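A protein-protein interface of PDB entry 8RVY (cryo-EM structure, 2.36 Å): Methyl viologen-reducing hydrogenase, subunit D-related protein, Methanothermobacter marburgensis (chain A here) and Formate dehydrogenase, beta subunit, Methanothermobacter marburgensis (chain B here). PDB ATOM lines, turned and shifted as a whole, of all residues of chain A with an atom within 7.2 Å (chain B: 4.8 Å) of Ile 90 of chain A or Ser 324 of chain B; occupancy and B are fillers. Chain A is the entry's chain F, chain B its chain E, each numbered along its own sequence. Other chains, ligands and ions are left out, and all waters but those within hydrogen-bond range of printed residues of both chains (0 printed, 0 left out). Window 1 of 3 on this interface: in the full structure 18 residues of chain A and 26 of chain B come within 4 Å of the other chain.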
ATOM      1  N   ASN A  46     -24.512  18.414  14.283  1.00  0.00           N
ATOM      2  CA  ASN A  46     -23.226  18.944  14.712  1.00  0.00           C
ATOM      3  C   ASN A  46     -23.158  20.425  14.358  1.00  0.00           C
ATOM      4  O   ASN A  46     -24.116  21.009  13.848  1.00  0.00           O
ATOM      5  CB  ASN A  46     -22.061  18.167  14.083  1.00  0.00           C
ATOM      6  CG  ASN A  46     -22.120  18.136  12.576  1.00  0.00           C
ATOM      7  OD1 ASN A  46     -22.918  18.832  11.960  1.00  0.00           O
ATOM      8  ND2 ASN A  46     -21.266  17.327  11.972  1.00  0.00           N
ATOM      9  N   ALA A  47     -22.008  21.036  14.644  1.00  0.00           N
ATOM     10  CA  ALA A  47     -21.852  22.467  14.410  1.00  0.00           C
ATOM     11  C   ALA A  47     -21.846  22.805  12.928  1.00  0.00           C
ATOM     12  O   ALA A  47     -22.237  23.911  12.551  1.00  0.00           O
ATOM     13  CB  ALA A  47     -20.568  22.968  15.061  1.00  0.00           C
ATOM     14  N   SER A  48     -21.404  21.877  12.076  1.00  0.00           N
ATOM     15  CA  SER A  48     -21.374  22.150  10.645  1.00  0.00           C
ATOM     16  C   SER A  48     -22.765  22.468  10.116  1.00  0.00           C
ATOM     17  O   SER A  48     -22.933  23.386   9.309  1.00  0.00           O
ATOM     18  CB  SER A  48     -20.778  20.962   9.896  1.00  0.00           C
ATOM     19  OG  SER A  48     -19.380  20.890  10.088  1.00  0.00           O
ATOM     20  N   LEU A  51     -23.800  26.035  11.383  1.00  0.00           N
ATOM     21  CA  LEU A  51     -23.041  27.072  10.699  1.00  0.00           C
ATOM     22  C   LEU A  51     -23.461  27.188   9.241  1.00  0.00           C
ATOM     23  O   LEU A  51     -23.542  28.296   8.704  1.00  0.00           O
ATOM     24  CB  LEU A  51     -21.546  26.780  10.809  1.00  0.00           C
ATOM     25  CG  LEU A  51     -20.998  26.753  12.234  1.00  0.00           C
ATOM     26  CD1 LEU A  51     -19.631  26.100  12.271  1.00  0.00           C
ATOM     27  CD2 LEU A  51     -20.943  28.151  12.807  1.00  0.00           C
ATOM     28  N   ARG A  83     -22.248  19.404  22.185  1.00  0.00           N
ATOM     29  CA  ARG A  83     -21.986  20.171  20.976  1.00  0.00           C
ATOM     30  C   ARG A  83     -22.719  21.502  21.002  1.00  0.00           C
ATOM     31  O   ARG A  83     -22.198  22.509  20.527  1.00  0.00           O
ATOM     32  CB  ARG A  83     -22.389  19.364  19.745  1.00  0.00           C
ATOM     33  CG  ARG A  83     -21.609  18.089  19.559  1.00  0.00           C
ATOM     34  CD  ARG A  83     -22.172  17.278  18.421  1.00  0.00           C
ATOM     35  NE  ARG A  83     -21.634  15.924  18.399  1.00  0.00           N
ATOM     36  CZ  ARG A  83     -22.322  14.845  18.060  1.00  0.00           C
ATOM     37  NH1 ARG A  83     -23.592  14.916  17.698  1.00  0.00           N
ATOM     38  NH2 ARG A  83     -21.721  13.660  18.084  1.00  0.00           N
ATOM     39  N   ALA A  84     -23.937  21.521  21.544  1.00  0.00           N
ATOM     40  CA  ALA A  84     -24.733  22.742  21.579  1.00  0.00           C
ATOM     41  C   ALA A  84     -24.111  23.784  22.498  1.00  0.00           C
ATOM     42  O   ALA A  84     -24.110  24.977  22.180  1.00  0.00           O
ATOM     43  CB  ALA A  84     -26.158  22.424  22.022  1.00  0.00           C
ATOM     44  N   ARG A  85     -23.589  23.358  23.649  1.00  0.00           N
ATOM     45  CA  ARG A  85     -22.897  24.307  24.516  1.00  0.00           C
ATOM     46  C   ARG A  85     -21.664  24.875  23.822  1.00  0.00           C
ATOM     47  O   ARG A  85     -21.415  26.091  23.859  1.00  0.00           O
ATOM     48  CB  ARG A  85     -22.510  23.638  25.834  1.00  0.00           C
ATOM     49  CG  ARG A  85     -23.612  23.582  26.885  1.00  0.00           C
ATOM     50  CD  ARG A  85     -24.215  24.952  27.215  1.00  0.00           C
ATOM     51  NE  ARG A  85     -23.306  26.064  26.958  1.00  0.00           N
ATOM     52  CZ  ARG A  85     -22.723  26.807  27.890  1.00  0.00           C
ATOM     53  NH1 ARG A  85     -22.910  26.580  29.180  1.00  0.00           N
ATOM     54  NH2 ARG A  85     -21.928  27.807  27.517  1.00  0.00           N
ATOM     55  N   PHE A  86     -20.888  24.015  23.161  1.00  0.00           N
ATOM     56  CA  PHE A  86     -19.719  24.519  22.446  1.00  0.00           C
ATOM     57  C   PHE A  86     -20.127  25.462  21.315  1.00  0.00           C
ATOM     58  O   PHE A  86     -19.444  26.457  21.048  1.00  0.00           O
ATOM     59  CB  PHE A  86     -18.886  23.354  21.913  1.00  0.00           C
ATOM     60  CG  PHE A  86     -17.479  23.729  21.533  1.00  0.00           C
ATOM     61  CD1 PHE A  86     -16.747  24.623  22.295  1.00  0.00           C
ATOM     62  CD2 PHE A  86     -16.886  23.179  20.412  1.00  0.00           C
ATOM     63  CE1 PHE A  86     -15.459  24.960  21.942  1.00  0.00           C
ATOM     64  CE2 PHE A  86     -15.599  23.517  20.057  1.00  0.00           C
ATOM     65  CZ  PHE A  86     -14.886  24.406  20.822  1.00  0.00           C
ATOM     66  N   ILE A  87     -21.240  25.172  20.642  1.00  0.00           N
ATOM     67  CA  ILE A  87     -21.711  26.033  19.563  1.00  0.00           C
ATOM     68  C   ILE A  87     -22.159  27.378  20.111  1.00  0.00           C
ATOM     69  O   ILE A  87     -21.992  28.414  19.462  1.00  0.00           O
ATOM     70  CB  ILE A  87     -22.844  25.345  18.780  1.00  0.00           C
ATOM     71  CG1 ILE A  87     -22.300  24.175  17.963  1.00  0.00           C
ATOM     72  CG2 ILE A  87     -23.534  26.340  17.865  1.00  0.00           C
ATOM     73  CD1 ILE A  87     -23.353  23.173  17.573  1.00  0.00           C
ATOM     74  N   GLU A  88     -22.770  27.384  21.295  1.00  0.00           N
ATOM     75  CA  GLU A  88     -23.113  28.648  21.932  1.00  0.00           C
ATOM     76  C   GLU A  88     -21.862  29.456  22.232  1.00  0.00           C
ATOM     77  O   GLU A  88     -21.867  30.688  22.134  1.00  0.00           O
ATOM     78  CB  GLU A  88     -23.902  28.397  23.214  1.00  0.00           C
ATOM     79  CG  GLU A  88     -25.395  28.534  23.056  1.00  0.00           C
ATOM     80  CD  GLU A  88     -26.148  27.917  24.209  1.00  0.00           C
ATOM     81  OE1 GLU A  88     -25.511  27.612  25.236  1.00  0.00           O
ATOM     82  OE2 GLU A  88     -27.375  27.737  24.089  1.00  0.00           O
ATOM     83  N   ASP A  89     -20.781  28.779  22.622  1.00  0.00           N
ATOM     84  CA  ASP A  89     -19.506  29.475  22.782  1.00  0.00           C
ATOM     85  C   ASP A  89     -19.016  30.054  21.456  1.00  0.00           C
ATOM     86  O   ASP A  89     -18.541  31.193  21.403  1.00  0.00           O
ATOM     87  CB  ASP A  89     -18.455  28.527  23.358  1.00  0.00           C
ATOM     88  CG  ASP A  89     -18.580  28.354  24.855  1.00  0.00           C
ATOM     89  OD1 ASP A  89     -19.358  29.098  25.485  1.00  0.00           O
ATOM     90  OD2 ASP A  89     -17.894  27.472  25.406  1.00  0.00           O
ATOM     91  N   ILE A  90     -19.117  29.278  20.377  1.00  0.00           N
ATOM     92  CA  ILE A  90     -18.516  29.675  19.104  1.00  0.00           C
ATOM     93  C   ILE A  90     -19.299  30.810  18.446  1.00  0.00           C
ATOM     94  O   ILE A  90     -18.710  31.741  17.888  1.00  0.00           O
ATOM     95  CB  ILE A  90     -18.406  28.457  18.168  1.00  0.00           C
ATOM     96  CG1 ILE A  90     -17.244  27.559  18.589  1.00  0.00           C
ATOM     97  CG2 ILE A  90     -18.212  28.900  16.729  1.00  0.00           C
ATOM     98  CD1 ILE A  90     -17.395  26.128  18.140  1.00  0.00           C
ATOM     99  N   LEU A  91     -20.629  30.750  18.486  1.00  0.00           N
ATOM    100  CA  LEU A  91     -21.443  31.591  17.609  1.00  0.00           C
ATOM    101  C   LEU A  91     -21.224  33.083  17.811  1.00  0.00           C
ATOM    102  O   LEU A  91     -21.093  33.804  16.809  1.00  0.00           O
ATOM    103  CB  LEU A  91     -22.921  31.234  17.792  1.00  0.00           C
ATOM    104  CG  LEU A  91     -23.470  30.114  16.910  1.00  0.00           C
ATOM    105  CD1 LEU A  91     -24.864  29.740  17.357  1.00  0.00           C
ATOM    106  CD2 LEU A  91     -23.471  30.515  15.453  1.00  0.00           C
ATOM    107  N   PRO A  92     -21.203  33.618  19.034  1.00  0.00           N
ATOM    108  CA  PRO A  92     -21.038  35.073  19.188  1.00  0.00           C
ATOM    109  C   PRO A  92     -19.715  35.601  18.660  1.00  0.00           C
ATOM    110  O   PRO A  92     -19.609  36.806  18.399  1.00  0.00           O
ATOM    111  CB  PRO A  92     -21.157  35.281  20.703  1.00  0.00           C
ATOM    112  CG  PRO A  92     -21.861  34.081  21.204  1.00  0.00           C
ATOM    113  CD  PRO A  92     -21.443  32.956  20.325  1.00  0.00           C
ATOM    114  N   GLU A  93     -18.703  34.749  18.494  1.00  0.00           N
ATOM    115  CA  GLU A  93     -17.421  35.215  17.984  1.00  0.00           C
ATOM    116  C   GLU A  93     -17.520  35.723  16.556  1.00  0.00           C
ATOM    117  O   GLU A  93     -16.611  36.418  16.093  1.00  0.00           O
ATOM    118  CB  GLU A  93     -16.386  34.094  18.046  1.00  0.00           C
ATOM    119  CG  GLU A  93     -16.050  33.641  19.445  1.00  0.00           C
ATOM    120  CD  GLU A  93     -15.384  34.716  20.274  1.00  0.00           C
ATOM    121  OE1 GLU A  93     -15.089  34.451  21.457  1.00  0.00           O
ATOM    122  OE2 GLU A  93     -15.138  35.818  19.746  1.00  0.00           O
ATOM    123  N   PHE A  94     -18.597  35.390  15.846  1.00  0.00           N
ATOM    124  CA  PHE A  94     -18.787  35.807  14.464  1.00  0.00           C
ATOM    125  C   PHE A  94     -20.028  36.676  14.299  1.00  0.00           C
ATOM    126  O   PHE A  94     -20.580  36.759  13.199  1.00  0.00           O
ATOM    127  CB  PHE A  94     -18.856  34.582  13.554  1.00  0.00           C
ATOM    128  CG  PHE A  94     -17.612  33.741  13.590  1.00  0.00           C
ATOM    129  CD1 PHE A  94     -16.569  33.987  12.716  1.00  0.00           C
ATOM    130  CD2 PHE A  94     -17.480  32.717  14.509  1.00  0.00           C
ATOM    131  CE1 PHE A  94     -15.426  33.224  12.756  1.00  0.00           C
ATOM    132  CE2 PHE A  94     -16.336  31.952  14.551  1.00  0.00           C
ATOM    133  CZ  PHE A  94     -15.308  32.208  13.674  1.00  0.00           C
ATOM    134  N   GLY A  95     -20.475  37.323  15.370  1.00  0.00           N
ATOM    135  CA  GLY A  95     -21.554  38.283  15.286  1.00  0.00           C
ATOM    136  C   GLY A  95     -22.949  37.705  15.310  1.00  0.00           C
ATOM    137  O   GLY A  95     -23.898  38.420  14.972  1.00  0.00           O
ATOM    138  N   ILE A  96     -23.111  36.445  15.696  1.00  0.00           N
ATOM    139  CA  ILE A  96     -24.417  35.802  15.752  1.00  0.00           C
ATOM    140  C   ILE A  96     -24.848  35.760  17.213  1.00  0.00           C
ATOM    141  O   ILE A  96     -24.241  35.062  18.030  1.00  0.00           O
ATOM    142  CB  ILE A  96     -24.381  34.397  15.136  1.00  0.00           C
ATOM    143  CG1 ILE A  96     -24.108  34.487  13.634  1.00  0.00           C
ATOM    144  CG2 ILE A  96     -25.687  33.668  15.388  1.00  0.00           C
ATOM    145  CD1 ILE A  96     -23.584  33.216  13.034  1.00  0.00           C
ATOM    146  N   GLY B 320     -15.385  28.915  11.804  1.00  0.00           N
ATOM    147  CA  GLY B 320     -16.249  28.322  12.801  1.00  0.00           C
ATOM    148  C   GLY B 320     -16.273  26.813  12.714  1.00  0.00           C
ATOM    149  O   GLY B 320     -16.384  26.135  13.734  1.00  0.00           O
ATOM    150  N   VAL B 321     -16.158  26.267  11.504  1.00  0.00           N
ATOM    151  CA  VAL B 321     -16.118  24.817  11.357  1.00  0.00           C
ATOM    152  C   VAL B 321     -14.820  24.262  11.931  1.00  0.00           C
ATOM    153  O   VAL B 321     -14.830  23.281  12.683  1.00  0.00           O
ATOM    154  CB  VAL B 321     -16.308  24.414   9.885  1.00  0.00           C
ATOM    155  CG1 VAL B 321     -16.140  22.917   9.717  1.00  0.00           C
ATOM    156  CG2 VAL B 321     -17.673  24.838   9.397  1.00  0.00           C
ATOM    157  N   ARG B 322     -13.680  24.877  11.599  1.00  0.00           N
ATOM    158  CA  ARG B 322     -12.432  24.405  12.195  1.00  0.00           C
ATOM    159  C   ARG B 322     -12.455  24.551  13.714  1.00  0.00           C
ATOM    160  O   ARG B 322     -11.901  23.707  14.432  1.00  0.00           O
ATOM    161  CB  ARG B 322     -11.242  25.153  11.599  1.00  0.00           C
ATOM    162  CG  ARG B 322      -9.914  24.443  11.791  1.00  0.00           C
ATOM    163  CD  ARG B 322      -8.830  24.977  10.871  1.00  0.00           C
ATOM    164  NE  ARG B 322      -8.114  26.107  11.450  1.00  0.00           N
ATOM    165  CZ  ARG B 322      -7.213  26.016  12.418  1.00  0.00           C
ATOM    166  NH1 ARG B 322      -6.887  24.852  12.952  1.00  0.00           N
ATOM    167  NH2 ARG B 322      -6.621  27.118  12.859  1.00  0.00           N
ATOM    168  N   LEU B 323     -13.101  25.602  14.219  1.00  0.00           N
ATOM    169  CA  LEU B 323     -13.227  25.787  15.659  1.00  0.00           C
ATOM    170  C   LEU B 323     -14.061  24.678  16.277  1.00  0.00           C
ATOM    171  O   LEU B 323     -13.626  24.024  17.223  1.00  0.00           O
ATOM    172  CB  LEU B 323     -13.846  27.150  15.961  1.00  0.00           C
ATOM    173  CG  LEU B 323     -12.888  28.337  15.960  1.00  0.00           C
ATOM    174  CD1 LEU B 323     -13.633  29.605  15.617  1.00  0.00           C
ATOM    175  CD2 LEU B 323     -12.188  28.466  17.297  1.00  0.00           C
ATOM    176  N   SER B 324     -15.247  24.425  15.734  1.00  0.00           N
ATOM    177  CA  SER B 324     -16.056  23.325  16.238  1.00  0.00           C
ATOM    178  C   SER B 324     -15.303  22.005  16.164  1.00  0.00           C
ATOM    179  O   SER B 324     -15.544  21.109  16.977  1.00  0.00           O
ATOM    180  CB  SER B 324     -17.362  23.237  15.453  1.00  0.00           C
ATOM    181  OG  SER B 324     -17.220  22.408  14.318  1.00  0.00           O
ATOM    182  N   HIS B 325     -14.389  21.868  15.203  1.00  0.00           N
ATOM    183  CA  HIS B 325     -13.649  20.621  15.058  1.00  0.00           C
ATOM    184  C   HIS B 325     -12.569  20.454  16.121  1.00  0.00           C
ATOM    185  O   HIS B 325     -12.397  19.353  16.652  1.00  0.00           O
ATOM    186  CB  HIS B 325     -13.017  20.545  13.673  1.00  0.00           C
ATOM    187  CG  HIS B 325     -13.947  20.055  12.611  1.00  0.00           C
ATOM    188  ND1 HIS B 325     -13.502  19.448  11.458  1.00  0.00           N
ATOM    189  CD2 HIS B 325     -15.295  20.089  12.523  1.00  0.00           C
ATOM    190  CE1 HIS B 325     -14.539  19.125  10.708  1.00  0.00           C
ATOM    191  NE2 HIS B 325     -15.638  19.504  11.331  1.00  0.00           N
ATOM    192  N   MET B 326     -11.807  21.510  16.425  1.00  0.00           N
ATOM    193  CA  MET B 326     -10.626  21.328  17.266  1.00  0.00           C
ATOM    194  C   MET B 326     -10.346  22.426  18.285  1.00  0.00           C
ATOM    195  O   MET B 326      -9.326  22.340  18.970  1.00  0.00           O
ATOM    196  CB  MET B 326      -9.372  21.153  16.382  1.00  0.00           C
ATOM    197  CG  MET B 326      -9.197  22.180  15.265  1.00  0.00           C
ATOM    198  SD  MET B 326      -8.870  23.866  15.822  1.00  0.00           S
ATOM    199  CE  MET B 326      -7.282  23.672  16.624  1.00  0.00           C
ATOM    200  N   PHE B 328     -11.304  23.154  21.184  1.00  0.00           N
ATOM    201  CA  PHE B 328     -11.078  22.687  22.544  1.00  0.00           C
ATOM    202  C   PHE B 328      -9.694  22.082  22.727  1.00  0.00           C
ATOM    203  O   PHE B 328      -9.274  21.871  23.867  1.00  0.00           O
ATOM    204  CB  PHE B 328     -12.146  21.661  22.943  1.00  0.00           C
ATOM    205  CG  PHE B 328     -12.529  20.720  21.841  1.00  0.00           C
ATOM    206  CD1 PHE B 328     -11.681  19.699  21.460  1.00  0.00           C
ATOM    207  CD2 PHE B 328     -13.730  20.866  21.173  1.00  0.00           C
ATOM    208  CE1 PHE B 328     -12.024  18.844  20.445  1.00  0.00           C
ATOM    209  CE2 PHE B 328     -14.076  20.011  20.156  1.00  0.00           C
ATOM    210  CZ  PHE B 328     -13.223  19.000  19.793  1.00  0.00           C
ATOM    211  N   ILE B 353     -11.453  30.845  22.386  1.00  0.00           N
ATOM    212  CA  ILE B 353     -12.467  29.797  22.401  1.00  0.00           C
ATOM    213  C   ILE B 353     -12.015  28.627  23.266  1.00  0.00           C
ATOM    214  O   ILE B 353     -12.803  28.065  24.040  1.00  0.00           O
ATOM    215  CB  ILE B 353     -12.790  29.353  20.963  1.00  0.00           C
ATOM    216  CG1 ILE B 353     -13.625  30.417  20.246  1.00  0.00           C
ATOM    217  CG2 ILE B 353     -13.506  28.016  20.959  1.00  0.00           C
ATOM    218  CD1 ILE B 353     -14.921  30.758  20.932  1.00  0.00           C
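Ile 90 of chain A touches just one residue of chain B: Ser 324. Of chain A, only Ala 47, Phe 86 and Ile 90 come within 4 Å of Ser 324 of chain B. Of the printed residues of chain B, Ser 48 of chain A touches Val 321. Of the printed residues of chain B, Asp 89 of chain A touches Ile 353 (3.7 Å). Of the printed residues of chain A, Phe 328 of chain B touches Phe 86. Of the printed residues of chain A, Gly 320 of chain B touches Leu 51 (3.5 Å) and Phe 94 (3.8 Å). Of the printed residues of chain A, Ile 353 of chain B touches Phe 86, Asp 89 and Glu 93. Arg 85 of chain A touches none of the printed residues of chain B. Arg 83 of chain A touches none of the printed residues of chain B.
CB of Ser 324 of chain B touches CB of Ala 47 of chain A (3.2 Å). Ser 48 of chain A touches Val 321 of chain B. C of Gly 320 of chain B touches CD1 of Leu 51 of chain A, at 3.5 Å. CD1 of Leu 51 of chain A touches N of Val 321 of chain B, at 3.6 Å. Leu 323 of chain B touches Phe 86 of chain A (O to CE2, 3.5 Å). Ser 324 of chain B touches Phe 86 of chain A. Phe 86 of chain A touches Phe 328 of chain B (CE2 to CD2, 3.4 Å). CD1 of Ile 90 of chain A touches CA of Ser 324 of chain B, 3.6 Å away. CG of Glu 93 of chain A touches CD1 of Ile 353 of chain B, 3.4 Å away. Phe 94 of chain A touches Leu 323 of chain B (CZ to CD1, 3.7 Å).
Of the 9 printed residues of chain B, 6 touch a printed residue of chain A. Hydrophobic or aromatic side chains of chain B within 4 Å of the printed part of chain A: Val 321, Leu 323, Phe 328 and Ile 353. Of the 18 printed residues of chain A, 8 touch a printed residue of chain B. Printed residues of chain A that touch a printed residue of chain B: Ala 47, Ser 48, Leu 51, Phe 86, Asp 89, Ile 90, Glu 93 and Phe 94. Hydrophobic or aromatic side chains of chain A within 4 Å of the printed part of chain B: Ala 47, Leu 51, Phe 86, Ile 90 and Phe 94. Among the printed residues, 13 pairs touch across the chains. Among the printed residues, no Asp or Glu carboxylate lies within 4 Å of a Lys or Arg side-chain nitrogen of the other chain.
NH2 of Arg 85 of chain A is in salt-bridge range of OD1 of Asp 89 of chain A, at 3.5 Å. The backbone carbonyl oxygen (O) of Val 321 of chain B sits at hydrogen-bond distance from the side-chain hydroxyl (OG) of Ser 324 of chain B (3.0 Å). The backbone NH (N) of Ser 48 of chain A sits close to the side-chain amide oxygen (OD1) of Asn 46 of chain A.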
